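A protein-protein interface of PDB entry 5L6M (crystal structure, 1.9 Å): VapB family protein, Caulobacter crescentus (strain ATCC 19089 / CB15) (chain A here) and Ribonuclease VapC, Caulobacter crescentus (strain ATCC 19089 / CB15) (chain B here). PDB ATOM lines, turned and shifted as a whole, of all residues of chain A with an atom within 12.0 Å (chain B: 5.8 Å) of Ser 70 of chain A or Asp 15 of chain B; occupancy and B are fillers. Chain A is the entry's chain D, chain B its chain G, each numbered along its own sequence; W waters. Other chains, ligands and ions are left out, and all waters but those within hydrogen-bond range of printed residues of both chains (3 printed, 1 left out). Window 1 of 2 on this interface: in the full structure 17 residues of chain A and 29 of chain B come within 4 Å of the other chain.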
ATOM      1  N   LEU A  58     -15.339   6.896 -18.018  1.00  0.00           N
ATOM      2  CA  LEU A  58     -14.444   7.351 -16.955  1.00  0.00           C
ATOM      3  C   LEU A  58     -15.219   8.109 -15.894  1.00  0.00           C
ATOM      4  O   LEU A  58     -15.096   7.839 -14.695  1.00  0.00           O
ATOM      5  CB  LEU A  58     -13.335   8.249 -17.517  1.00  0.00           C
ATOM      6  CG  LEU A  58     -12.455   8.908 -16.436  1.00  0.00           C
ATOM      7  CD1 LEU A  58     -11.708   7.852 -15.607  1.00  0.00           C
ATOM      8  CD2 LEU A  58     -11.452   9.879 -17.072  1.00  0.00           C
ATOM      9  N   VAL A  59     -16.031   9.070 -16.323  1.00  0.00           N
ATOM     10  CA  VAL A  59     -16.745   9.896 -15.354  1.00  0.00           C
ATOM     11  C   VAL A  59     -17.740   9.063 -14.555  1.00  0.00           C
ATOM     12  O   VAL A  59     -17.914   9.275 -13.350  1.00  0.00           O
ATOM     13  CB  VAL A  59     -17.404  11.075 -16.077  1.00  0.00           C
ATOM     14  CG1 VAL A  59     -18.333  11.848 -15.138  1.00  0.00           C
ATOM     15  CG2 VAL A  59     -16.304  11.992 -16.624  1.00  0.00           C
ATOM     16  N   THR A  61     -17.356   5.930 -13.781  1.00  0.00           N
ATOM     17  CA  THR A  61     -16.569   5.214 -12.788  1.00  0.00           C
ATOM     18  C   THR A  61     -16.181   6.119 -11.621  1.00  0.00           C
ATOM     19  O   THR A  61     -16.257   5.707 -10.455  1.00  0.00           O
ATOM     20  CB  THR A  61     -15.346   4.600 -13.457  1.00  0.00           C
ATOM     21  OG1 THR A  61     -15.804   3.600 -14.372  1.00  0.00           O
ATOM     22  CG2 THR A  61     -14.430   3.947 -12.415  1.00  0.00           C
ATOM     23  N   LEU A  62     -15.740   7.343 -11.915  1.00  0.00           N
ATOM     24  CA  LEU A  62     -15.399   8.288 -10.856  1.00  0.00           C
ATOM     25  C   LEU A  62     -16.606   8.591  -9.975  1.00  0.00           C
ATOM     26  O   LEU A  62     -16.483   8.678  -8.741  1.00  0.00           O
ATOM     27  CB  LEU A  62     -14.855   9.589 -11.461  1.00  0.00           C
ATOM     28  CG  LEU A  62     -13.459   9.437 -12.091  1.00  0.00           C
ATOM     29  CD1 LEU A  62     -12.971  10.711 -12.853  1.00  0.00           C
ATOM     30  CD2 LEU A  62     -12.479   9.000 -10.959  1.00  0.00           C
ATOM     31  N   ASN A  63     -17.786   8.743 -10.585  1.00  0.00           N
ATOM     32  CA  ASN A  63     -18.962   9.116  -9.803  1.00  0.00           C
ATOM     33  C   ASN A  63     -19.480   7.986  -8.930  1.00  0.00           C
ATOM     34  O   ASN A  63     -20.224   8.259  -7.975  1.00  0.00           O
ATOM     35  CB  ASN A  63     -20.084   9.631 -10.724  1.00  0.00           C
ATOM     36  CG  ASN A  63     -19.768  11.002 -11.284  1.00  0.00           C
ATOM     37  OD1 ASN A  63     -18.920  11.713 -10.743  1.00  0.00           O
ATOM     38  ND2 ASN A  63     -20.437  11.382 -12.366  1.00  0.00           N
ATOM     39  N   GLN A  64     -19.120   6.734  -9.230  1.00  0.00           N
ATOM     40  CA  GLN A  64     -19.464   5.632  -8.343  1.00  0.00           C
ATOM     41  C   GLN A  64     -18.563   5.567  -7.123  1.00  0.00           C
ATOM     42  O   GLN A  64     -18.924   4.922  -6.133  1.00  0.00           O
ATOM     43  CB  GLN A  64     -19.393   4.310  -9.093  1.00  0.00           C
ATOM     44  CG  GLN A  64     -20.344   4.250 -10.267  1.00  0.00           C
ATOM     45  CD  GLN A  64     -20.045   3.049 -11.117  1.00  0.00           C
ATOM     46  OE1 GLN A  64     -18.882   2.791 -11.464  1.00  0.00           O
ATOM     47  NE2 GLN A  64     -21.071   2.269 -11.403  1.00  0.00           N
ATOM     48  N   MET A  65     -17.442   6.214  -7.172  1.00  0.00           N
ATOM     49  CA  MET A  65     -16.494   6.196  -6.075  1.00  0.00           C
ATOM     50  C   MET A  65     -16.748   7.369  -5.135  1.00  0.00           C
ATOM     51  O   MET A  65     -17.151   8.441  -5.582  1.00  0.00           O
ATOM     52  CB  MET A  65     -15.070   6.281  -6.623  1.00  0.00           C
ATOM     53  CG  MET A  65     -14.734   5.165  -7.604  1.00  0.00           C
ATOM     54  SD  MET A  65     -13.182   5.509  -8.461  1.00  0.00           S
ATOM     55  CE  MET A  65     -12.032   5.089  -7.179  1.00  0.00           C
ATOM     56  N   PRO A  66     -16.499   7.232  -3.830  1.00  0.00           N
ATOM     57  CA  PRO A  66     -16.652   8.387  -2.936  1.00  0.00           C
ATOM     58  C   PRO A  66     -15.812   9.562  -3.411  1.00  0.00           C
ATOM     59  O   PRO A  66     -14.710   9.389  -3.931  1.00  0.00           O
ATOM     60  CB  PRO A  66     -16.144   7.865  -1.588  1.00  0.00           C
ATOM     61  CG  PRO A  66     -16.383   6.357  -1.671  1.00  0.00           C
ATOM     62  CD  PRO A  66     -16.105   6.012  -3.100  1.00  0.00           C
ATOM     63  N   ARG A  67     -16.321  10.723  -3.216  1.00  0.00           N
ATOM     64  CA  ARG A  67     -15.359  11.731  -3.597  1.00  0.00           C
ATOM     65  C   ARG A  67     -14.679  12.310  -2.366  1.00  0.00           C
ATOM     66  O   ARG A  67     -15.209  12.219  -1.254  1.00  0.00           O
ATOM     67  CB  ARG A  67     -16.029  12.852  -4.405  1.00  0.00           C
ATOM     68  CG  ARG A  67     -17.199  13.537  -3.754  1.00  0.00           C
ATOM     69  CD  ARG A  67     -17.286  14.958  -4.307  1.00  0.00           C
ATOM     70  NE  ARG A  67     -18.580  15.595  -4.087  1.00  0.00           N
ATOM     71  CZ  ARG A  67     -18.865  16.851  -4.435  1.00  0.00           C
ATOM     72  NH1 ARG A  67     -17.941  17.611  -5.009  1.00  0.00           N
ATOM     73  NH2 ARG A  67     -20.074  17.346  -4.210  1.00  0.00           N
ATOM     74  N   PRO A  68     -13.494  12.886  -2.546  1.00  0.00           N
ATOM     75  CA  PRO A  68     -12.734  13.392  -1.396  1.00  0.00           C
ATOM     76  C   PRO A  68     -13.491  14.510  -0.698  1.00  0.00           C
ATOM     77  O   PRO A  68     -14.359  15.168  -1.280  1.00  0.00           O
ATOM     78  CB  PRO A  68     -11.429  13.899  -2.027  1.00  0.00           C
ATOM     79  CG  PRO A  68     -11.333  13.131  -3.355  1.00  0.00           C
ATOM     80  CD  PRO A  68     -12.748  13.013  -3.819  1.00  0.00           C
ATOM     81  N   ASP A  69     -13.178  14.708   0.592  1.00  0.00           N
ATOM     82  CA  ASP A  69     -13.945  15.719   1.330  1.00  0.00           C
ATOM     83  C   ASP A  69     -13.570  17.144   0.940  1.00  0.00           C
ATOM     84  O   ASP A  69     -14.095  18.094   1.522  1.00  0.00           O
ATOM     85  CB  ASP A  69     -13.789  15.526   2.842  1.00  0.00           C
ATOM     86  CG  ASP A  69     -12.426  15.937   3.359  1.00  0.00           C
ATOM     87  OD1 ASP A  69     -11.492  16.124   2.553  1.00  0.00           O
ATOM     88  OD2 ASP A  69     -12.288  16.071   4.590  1.00  0.00           O
ATOM     89  N   SER A  70     -12.675  17.315  -0.027  1.00  0.00           N
ATOM     90  CA  SER A  70     -12.285  18.651  -0.445  1.00  0.00           C
ATOM     91  C   SER A  70     -11.719  18.531  -1.851  1.00  0.00           C
ATOM     92  O   SER A  70     -11.376  17.439  -2.302  1.00  0.00           O
ATOM     93  CB  SER A  70     -11.253  19.264   0.515  1.00  0.00           C
ATOM     94  OG  SER A  70     -10.015  18.561   0.405  1.00  0.00           O
ATOM     95  N   VAL A  71     -11.668  19.656  -2.549  1.00  0.00           N
ATOM     96  CA  VAL A  71     -10.977  19.755  -3.823  1.00  0.00           C
ATOM     97  C   VAL A  71      -9.649  20.445  -3.564  1.00  0.00           C
ATOM     98  O   VAL A  71      -9.612  21.576  -3.063  1.00  0.00           O
ATOM     99  CB  VAL A  71     -11.809  20.524  -4.858  1.00  0.00           C
ATOM    100  CG1 VAL A  71     -10.983  20.753  -6.110  1.00  0.00           C
ATOM    101  CG2 VAL A  71     -13.102  19.757  -5.157  1.00  0.00           C
ATOM    102  N   GLU A  72      -8.560  19.780  -3.915  1.00  0.00           N
ATOM    103  CA  GLU A  72      -7.243  20.297  -3.577  1.00  0.00           C
ATOM    104  C   GLU A  72      -6.952  21.575  -4.338  1.00  0.00           C
ATOM    105  O   GLU A  72      -7.401  21.762  -5.471  1.00  0.00           O
ATOM    106  CB  GLU A  72      -6.169  19.257  -3.897  1.00  0.00           C
ATOM    107  CG  GLU A  72      -5.722  18.534  -2.684  1.00  0.00           C
ATOM    108  CD  GLU A  72      -4.659  17.515  -2.989  1.00  0.00           C
ATOM    109  OE1 GLU A  72      -4.160  17.496  -4.132  1.00  0.00           O
ATOM    110  OE2 GLU A  72      -4.357  16.724  -2.081  1.00  0.00           O
ATOM    111  N   ILE A  73      -6.190  22.460  -3.703  1.00  0.00           N
ATOM    112  CA  ILE A  73      -5.716  23.658  -4.375  1.00  0.00           C
ATOM    113  C   ILE A  73      -4.437  23.338  -5.143  1.00  0.00           C
ATOM    114  O   ILE A  73      -3.603  22.546  -4.690  1.00  0.00           O
ATOM    115  CB  ILE A  73      -5.519  24.767  -3.334  1.00  0.00           C
ATOM    116  CG1 ILE A  73      -6.893  25.203  -2.809  1.00  0.00           C
ATOM    117  CG2 ILE A  73      -4.761  25.934  -3.921  1.00  0.00           C
ATOM    118  CD1 ILE A  73      -6.837  25.789  -1.431  1.00  0.00           C
ATOM    119  N   ARG A  74      -4.289  23.918  -6.335  1.00  0.00           N
ATOM    120  CA  ARG A  74      -3.082  23.696  -7.135  1.00  0.00           C
ATOM    121  C   ARG A  74      -1.921  24.482  -6.537  1.00  0.00           C
ATOM    122  O   ARG A  74      -1.886  25.718  -6.613  1.00  0.00           O
ATOM    123  CB  ARG A  74      -3.308  24.111  -8.580  1.00  0.00           C
ATOM    124  CG  ARG A  74      -2.062  23.976  -9.421  1.00  0.00           C
ATOM    125  CD  ARG A  74      -2.363  24.221 -10.861  1.00  0.00           C
ATOM    126  NE  ARG A  74      -1.228  23.862 -11.721  1.00  0.00           N
ATOM    127  CZ  ARG A  74      -0.588  24.710 -12.513  1.00  0.00           C
ATOM    128  NH1 ARG A  74      -0.985  25.973 -12.573  1.00  0.00           N
ATOM    129  NH2 ARG A  74       0.425  24.296 -13.262  1.00  0.00           N
ATOM    130  N   ASP A  75      -0.958  23.771  -5.955  1.00  0.00           N
ATOM    131  CA  ASP A  75       0.105  24.446  -5.215  1.00  0.00           C
ATOM    132  C   ASP A  75       0.981  25.299  -6.128  1.00  0.00           C
ATOM    133  O   ASP A  75       1.538  26.317  -5.691  1.00  0.00           O
ATOM    134  CB  ASP A  75       0.927  23.402  -4.454  1.00  0.00           C
ATOM    135  CG  ASP A  75       1.646  23.984  -3.248  1.00  0.00           C
ATOM    136  OD1 ASP A  75       1.084  24.867  -2.563  1.00  0.00           O
ATOM    137  OD2 ASP A  75       2.782  23.551  -2.987  1.00  0.00           O
ATOM    138  N   ALA B  10      -7.922  19.019 -14.211  1.00  0.00           N
ATOM    139  CA  ALA B  10      -7.697  17.615 -13.864  1.00  0.00           C
ATOM    140  C   ALA B  10      -7.747  17.393 -12.350  1.00  0.00           C
ATOM    141  O   ALA B  10      -8.173  16.323 -11.897  1.00  0.00           O
ATOM    142  CB  ALA B  10      -6.351  17.125 -14.437  1.00  0.00           C
ATOM    143  N   ILE B  11      -7.314  18.375 -11.556  1.00  0.00           N
ATOM    144  CA  ILE B  11      -7.478  18.244 -10.109  1.00  0.00           C
ATOM    145  C   ILE B  11      -8.958  18.149  -9.772  1.00  0.00           C
ATOM    146  O   ILE B  11      -9.389  17.269  -9.014  1.00  0.00           O
ATOM    147  CB  ILE B  11      -6.825  19.426  -9.373  1.00  0.00           C
ATOM    148  CG1 ILE B  11      -5.303  19.381  -9.489  1.00  0.00           C
ATOM    149  CG2 ILE B  11      -7.251  19.441  -7.887  1.00  0.00           C
ATOM    150  CD1 ILE B  11      -4.664  20.601  -8.864  1.00  0.00           C
ATOM    151  N   HIS B  12      -9.760  19.045 -10.362  1.00  0.00           N
ATOM    152  CA  HIS B  12     -11.182  19.086 -10.046  1.00  0.00           C
ATOM    153  C   HIS B  12     -11.880  17.819 -10.518  1.00  0.00           C
ATOM    154  O   HIS B  12     -12.818  17.355  -9.863  1.00  0.00           O
ATOM    155  CB  HIS B  12     -11.810  20.345 -10.660  1.00  0.00           C
ATOM    156  CG  HIS B  12     -11.555  21.597  -9.868  1.00  0.00           C
ATOM    157  ND1 HIS B  12     -12.569  22.426  -9.443  1.00  0.00           N
ATOM    158  CD2 HIS B  12     -10.403  22.152  -9.414  1.00  0.00           C
ATOM    159  CE1 HIS B  12     -12.057  23.443  -8.769  1.00  0.00           C
ATOM    160  NE2 HIS B  12     -10.745  23.293  -8.726  1.00  0.00           N
ATOM    161  N   LEU B  13     -11.415  17.222 -11.624  1.00  0.00           N
ATOM    162  CA  LEU B  13     -11.954  15.927 -12.042  1.00  0.00           C
ATOM    163  C   LEU B  13     -11.581  14.830 -11.046  1.00  0.00           C
ATOM    164  O   LEU B  13     -12.450  14.082 -10.586  1.00  0.00           O
ATOM    165  CB  LEU B  13     -11.470  15.575 -13.452  1.00  0.00           C
ATOM    166  CG  LEU B  13     -11.835  14.228 -14.093  1.00  0.00           C
ATOM    167  CD1 LEU B  13     -13.344  14.086 -14.198  1.00  0.00           C
ATOM    168  CD2 LEU B  13     -11.192  14.164 -15.482  1.00  0.00           C
ATOM    169  N   ARG B  14     -10.288  14.709 -10.713  1.00  0.00           N
ATOM    170  CA  ARG B  14      -9.863  13.725  -9.723  1.00  0.00           C
ATOM    171  C   ARG B  14     -10.660  13.849  -8.427  1.00  0.00           C
ATOM    172  O   ARG B  14     -11.107  12.838  -7.872  1.00  0.00           O
ATOM    173  CB  ARG B  14      -8.365  13.857  -9.428  1.00  0.00           C
ATOM    174  CG  ARG B  14      -7.788  12.682  -8.627  1.00  0.00           C
ATOM    175  CD  ARG B  14      -6.543  13.089  -7.815  1.00  0.00           C
ATOM    176  NE  ARG B  14      -6.752  14.297  -7.002  1.00  0.00           N
ATOM    177  CZ  ARG B  14      -5.753  15.074  -6.599  1.00  0.00           C
ATOM    178  NH1 ARG B  14      -4.496  14.745  -6.935  1.00  0.00           N
ATOM    179  NH2 ARG B  14      -5.999  16.179  -5.879  1.00  0.00           N
ATOM    180  N   ASP B  15     -10.873  15.074  -7.942  1.00  0.00           N
ATOM    181  CA  ASP B  15     -11.538  15.283  -6.662  1.00  0.00           C
ATOM    182  C   ASP B  15     -13.048  15.425  -6.769  1.00  0.00           C
ATOM    183  O   ASP B  15     -13.701  15.732  -5.764  1.00  0.00           O
ATOM    184  CB  ASP B  15     -10.924  16.481  -5.944  1.00  0.00           C
ATOM    185  CG  ASP B  15      -9.489  16.185  -5.474  1.00  0.00           C
ATOM    186  OD1 ASP B  15      -9.083  15.004  -5.521  1.00  0.00           O
ATOM    187  OD2 ASP B  15      -8.785  17.123  -5.065  1.00  0.00           O
ATOM    188  N   GLY B  16     -13.622  15.178  -7.943  1.00  0.00           N
ATOM    189  CA  GLY B  16     -15.062  15.025  -8.053  1.00  0.00           C
ATOM    190  C   GLY B  16     -15.879  16.299  -8.095  1.00  0.00           C
ATOM    191  O   GLY B  16     -17.043  16.284  -7.691  1.00  0.00           O
ATOM    192  N   ASP B  17     -15.306  17.404  -8.581  1.00  0.00           N
ATOM    193  CA  ASP B  17     -16.041  18.655  -8.751  1.00  0.00           C
ATOM    194  C   ASP B  17     -17.157  18.471  -9.775  1.00  0.00           C
ATOM    195  O   ASP B  17     -16.863  18.289 -10.965  1.00  0.00           O
ATOM    196  CB  ASP B  17     -15.090  19.771  -9.192  1.00  0.00           C
ATOM    197  CG  ASP B  17     -15.812  21.110  -9.450  1.00  0.00           C
ATOM    198  OD1 ASP B  17     -17.019  21.242  -9.166  1.00  0.00           O
ATOM    199  OD2 ASP B  17     -15.158  22.046  -9.946  1.00  0.00           O
ATOM    200  N   GLU B  48      -3.418  15.309   2.066  1.00  0.00           N
ATOM    201  CA  GLU B  48      -4.416  15.165   3.120  1.00  0.00           C
ATOM    202  C   GLU B  48      -4.484  13.675   3.432  1.00  0.00           C
ATOM    203  O   GLU B  48      -5.122  12.907   2.699  1.00  0.00           O
ATOM    204  CB  GLU B  48      -5.758  15.733   2.672  1.00  0.00           C
ATOM    205  CG  GLU B  48      -6.875  15.551   3.664  1.00  0.00           C
ATOM    206  CD  GLU B  48      -8.150  16.201   3.183  1.00  0.00           C
ATOM    207  OE1 GLU B  48      -9.092  16.332   4.000  1.00  0.00           O
ATOM    208  OE2 GLU B  48      -8.209  16.567   1.977  1.00  0.00           O
ATOM    209  N   GLN B  51      -7.407  11.290   3.240  1.00  0.00           N
ATOM    210  CA  GLN B  51      -8.000  11.121   1.910  1.00  0.00           C
ATOM    211  C   GLN B  51      -7.051  10.485   0.901  1.00  0.00           C
ATOM    212  O   GLN B  51      -7.379  10.444  -0.299  1.00  0.00           O
ATOM    213  CB  GLN B  51      -8.454  12.470   1.347  1.00  0.00           C
ATOM    214  CG  GLN B  51      -9.232  13.323   2.281  1.00  0.00           C
ATOM    215  CD  GLN B  51     -10.613  12.804   2.520  1.00  0.00           C
ATOM    216  OE1 GLN B  51     -11.416  12.694   1.600  1.00  0.00           O
ATOM    217  NE2 GLN B  51     -10.910  12.487   3.769  1.00  0.00           N
ATOM    218  N   ARG B  55      -7.829   9.501  -3.079  1.00  0.00           N
ATOM    219  CA  ARG B  55      -7.211  10.237  -4.170  1.00  0.00           C
ATOM    220  C   ARG B  55      -6.325   9.332  -5.008  1.00  0.00           C
ATOM    221  O   ARG B  55      -6.261   9.487  -6.236  1.00  0.00           O
ATOM    222  CB  ARG B  55      -6.412  11.416  -3.609  1.00  0.00           C
ATOM    223  CG  ARG B  55      -7.329  12.544  -3.172  1.00  0.00           C
ATOM    224  CD  ARG B  55      -6.573  13.821  -3.022  1.00  0.00           C
ATOM    225  NE  ARG B  55      -7.482  14.949  -2.996  1.00  0.00           N
ATOM    226  CZ  ARG B  55      -7.863  15.566  -1.883  1.00  0.00           C
ATOM    227  NH1 ARG B  55      -7.400  15.162  -0.707  1.00  0.00           N
ATOM    228  NH2 ARG B  55      -8.721  16.570  -1.950  1.00  0.00           N
ATOM    229  N   ARG B  58      -8.712   7.340  -7.252  1.00  0.00           N
ATOM    230  CA  ARG B  58      -9.328   8.188  -8.254  1.00  0.00           C
ATOM    231  C   ARG B  58      -8.304   8.627  -9.298  1.00  0.00           C
ATOM    232  O   ARG B  58      -8.585   8.603 -10.502  1.00  0.00           O
ATOM    233  CB  ARG B  58     -10.022   9.362  -7.532  1.00  0.00           C
ATOM    234  CG  ARG B  58     -11.258   8.843  -6.661  1.00  0.00           C
ATOM    235  CD  ARG B  58     -12.029   9.969  -5.939  1.00  0.00           C
ATOM    236  NE  ARG B  58     -12.490  10.867  -6.982  1.00  0.00           N
ATOM    237  CZ  ARG B  58     -13.723  10.891  -7.471  1.00  0.00           C
ATOM    238  NH1 ARG B  58     -14.671  10.113  -6.940  1.00  0.00           N
ATOM    239  NH2 ARG B  58     -13.995  11.707  -8.491  1.00  0.00           N
HETATM  240  O   HOH W   1     -11.755  14.114   6.648  1.00  0.00           O
HETATM  241  O   HOH W   2      -7.946  23.507  -7.287  1.00  0.00           O
HETATM  242  O   HOH W   3     -16.784  11.985  -9.263  1.00  0.00           O
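The side-chain carboxylate (OE2) of Glu 72 of chain A lies within salt-bridge range of the guanidinium group (NH1) of Arg 55 of chain B, at 3.7 Å. OD1 of Asp 69 of chain A lies close to OE1 of Glu 48 of chain B. The backbone carbonyl oxygen of Gly 16 of chain B is in hydrogen-bond range of the guanidinium group of Arg 67 of chain A (3.1 Å). The side-chain carboxylate (OE2) of Glu 48 of chain B sits at hydrogen-bond distance from the side-chain hydroxyl (OG) of Ser 70 of chain A, 3.1 Å away. The backbone carbonyl oxygen (O) of Pro 66 of chain A is in hydrogen-bond range of the guanidinium group (NH1) of Arg 58 of chain B. NH2 of Arg 14 of chain B lies within salt-bridge range of OE1 of Glu 72 of chain A (2.9 Å). The backbone carbonyl oxygen (O) of Met 65 of chain A sits at hydrogen-bond distance from the guanidinium group (NH1) of Arg 58 of chain B, at 3.3 Å. The side-chain carboxylate (OD2) of Asp 15 of chain B lies within hydrogen-bond range of the backbone NH (N) of Glu 72 of chain A, 2.9 Å away. The backbone NH (N) of Asp 69 of chain A lies within hydrogen-bond range of the side-chain amide oxygen (OE1) of Gln 51 of chain B (2.9 Å). O of Leu 62 of chain A sits at hydrogen-bond distance from NH1 of Arg 58 of chain B, 2.9 Å away. NH2 of Arg 55 of chain B lies within hydrogen-bond range of O of Ser 70 of chain A (2.8 Å).
OD1 of Asp 15 of chain B lies within salt-bridge range of NE of Arg 55 of chain B (3.0 Å). The guanidinium group (NH1) of Arg 55 of chain B lies within salt-bridge range of the side-chain carboxylate (OE2) of Glu 48 of chain B. OD2 of Asp 17 of chain B is in hydrogen-bond range of ND1 of His 12 of chain B (2.7 Å). The guanidinium group of Arg 14 of chain B is in salt-bridge range of the side-chain carboxylate of Asp 15 of chain B (2.9 Å). The backbone carbonyl oxygen (O) of Arg 14 of chain B lies within hydrogen-bond range of the guanidinium group (NE) of Arg 58 of chain B (2.6 Å).
CD1 of Leu 62 of chain A touches CD1 of Leu 13 of chain B, 3.7 Å away. Arg 58 of chain B touches Arg 67 of chain A (NH1 to CA, 3.8 Å). CD of Pro 68 of chain A touches O of Asp 15 of chain B, 3.5 Å away. Pro 68 of chain A touches Gln 51 of chain B. Pro 68 of chain A touches Arg 55 of chain B. Pro 68 of chain A touches Arg 58 of chain B (CD to CD, 3.8 Å). Asp 15 of chain B touches Ser 70 of chain A. Asp 15 of chain B touches Val 71 of chain A (OD2 to CA, 3.6 Å). O of Glu 72 of chain A touches CG2 of Ile 11 of chain B (3.4 Å). Arg 74 of chain A touches Ile 11 of chain B (CB to CD1, 3.8 Å).
Asn 63 of chain A touches none of the printed residues of chain B. Printed residues of chain B within 4 Å of Pro 68 of chain A: Asp 15, Gln 51, Arg 55 and Arg 58. Ser 70 of chain A touches three residues of chain B. Printed residues of chain B within 4 Å of Glu 72 of chain A: Ile 11, Arg 14, Asp 15 and Arg 55. Ala 10 of chain B touches none of the printed residues of chain A. Arg 14 of chain B touches just one residue of chain A: Glu 72. Asp 15 of chain B touches just these residues of chain A: Arg 67, Pro 68, Ser 70, Val 71 and Glu 72. Gly 16 of chain B touches just one residue of chain A: Arg 67. Asp 17 of chain B touches none of the printed residues of chain A. Of chain A, only Leu 62, Met 65, Pro 66, Arg 67 and Pro 68 come within 4 Å of Arg 58 of chain B. The nearest residue of chain B that does not touch Ser 70 of chain A is Gln 51 of chain B (5.1 Å). The nearest residue of chain A that does not touch Asp 15 of chain B is Ile 73 of chain A (6.1 Å).
Of the 12 printed residues of chain B, 10 touch a printed residue of chain A. Hydrophobic or aromatic side chains of chain B that line the printed part of chain A: Ile 11, His 12 and Leu 13. Hydrophobic or aromatic side chains of chain A that line the printed part of chain B: Leu 62, Met 65, Pro 68 and Val 71. Among the printed residues, 23 pairs touch across the chains. Among the printed residues, Asp or Glu carboxylates within 4 Å of a Lys or Arg side-chain nitrogen of the other chain: Glu 72 of chain A with Arg 14 of chain B (2.9 Å) and Glu 72 of chain A with Arg 55 of chain B (3.7 Å).
Water W2 lies within hydrogen-bond range of O of Glu 72 of chain A (2.6 Å) and NE2 of His 12 of chain B (3.2 Å). Water W3 lies within hydrogen-bond range of OD1 of Asn 63 of chain A (2.6 Å), NH2 of Arg 58 of chain B (2.9 Å) and O of Leu 62 of chain A (3.4 Å). Water W1 bridges the side-chain carboxylate (OD2) of Asp 69 of chain A (2.9 Å) and the side-chain amide nitrogen (NE2) of Gln 51 of chain B (3.4 Å).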
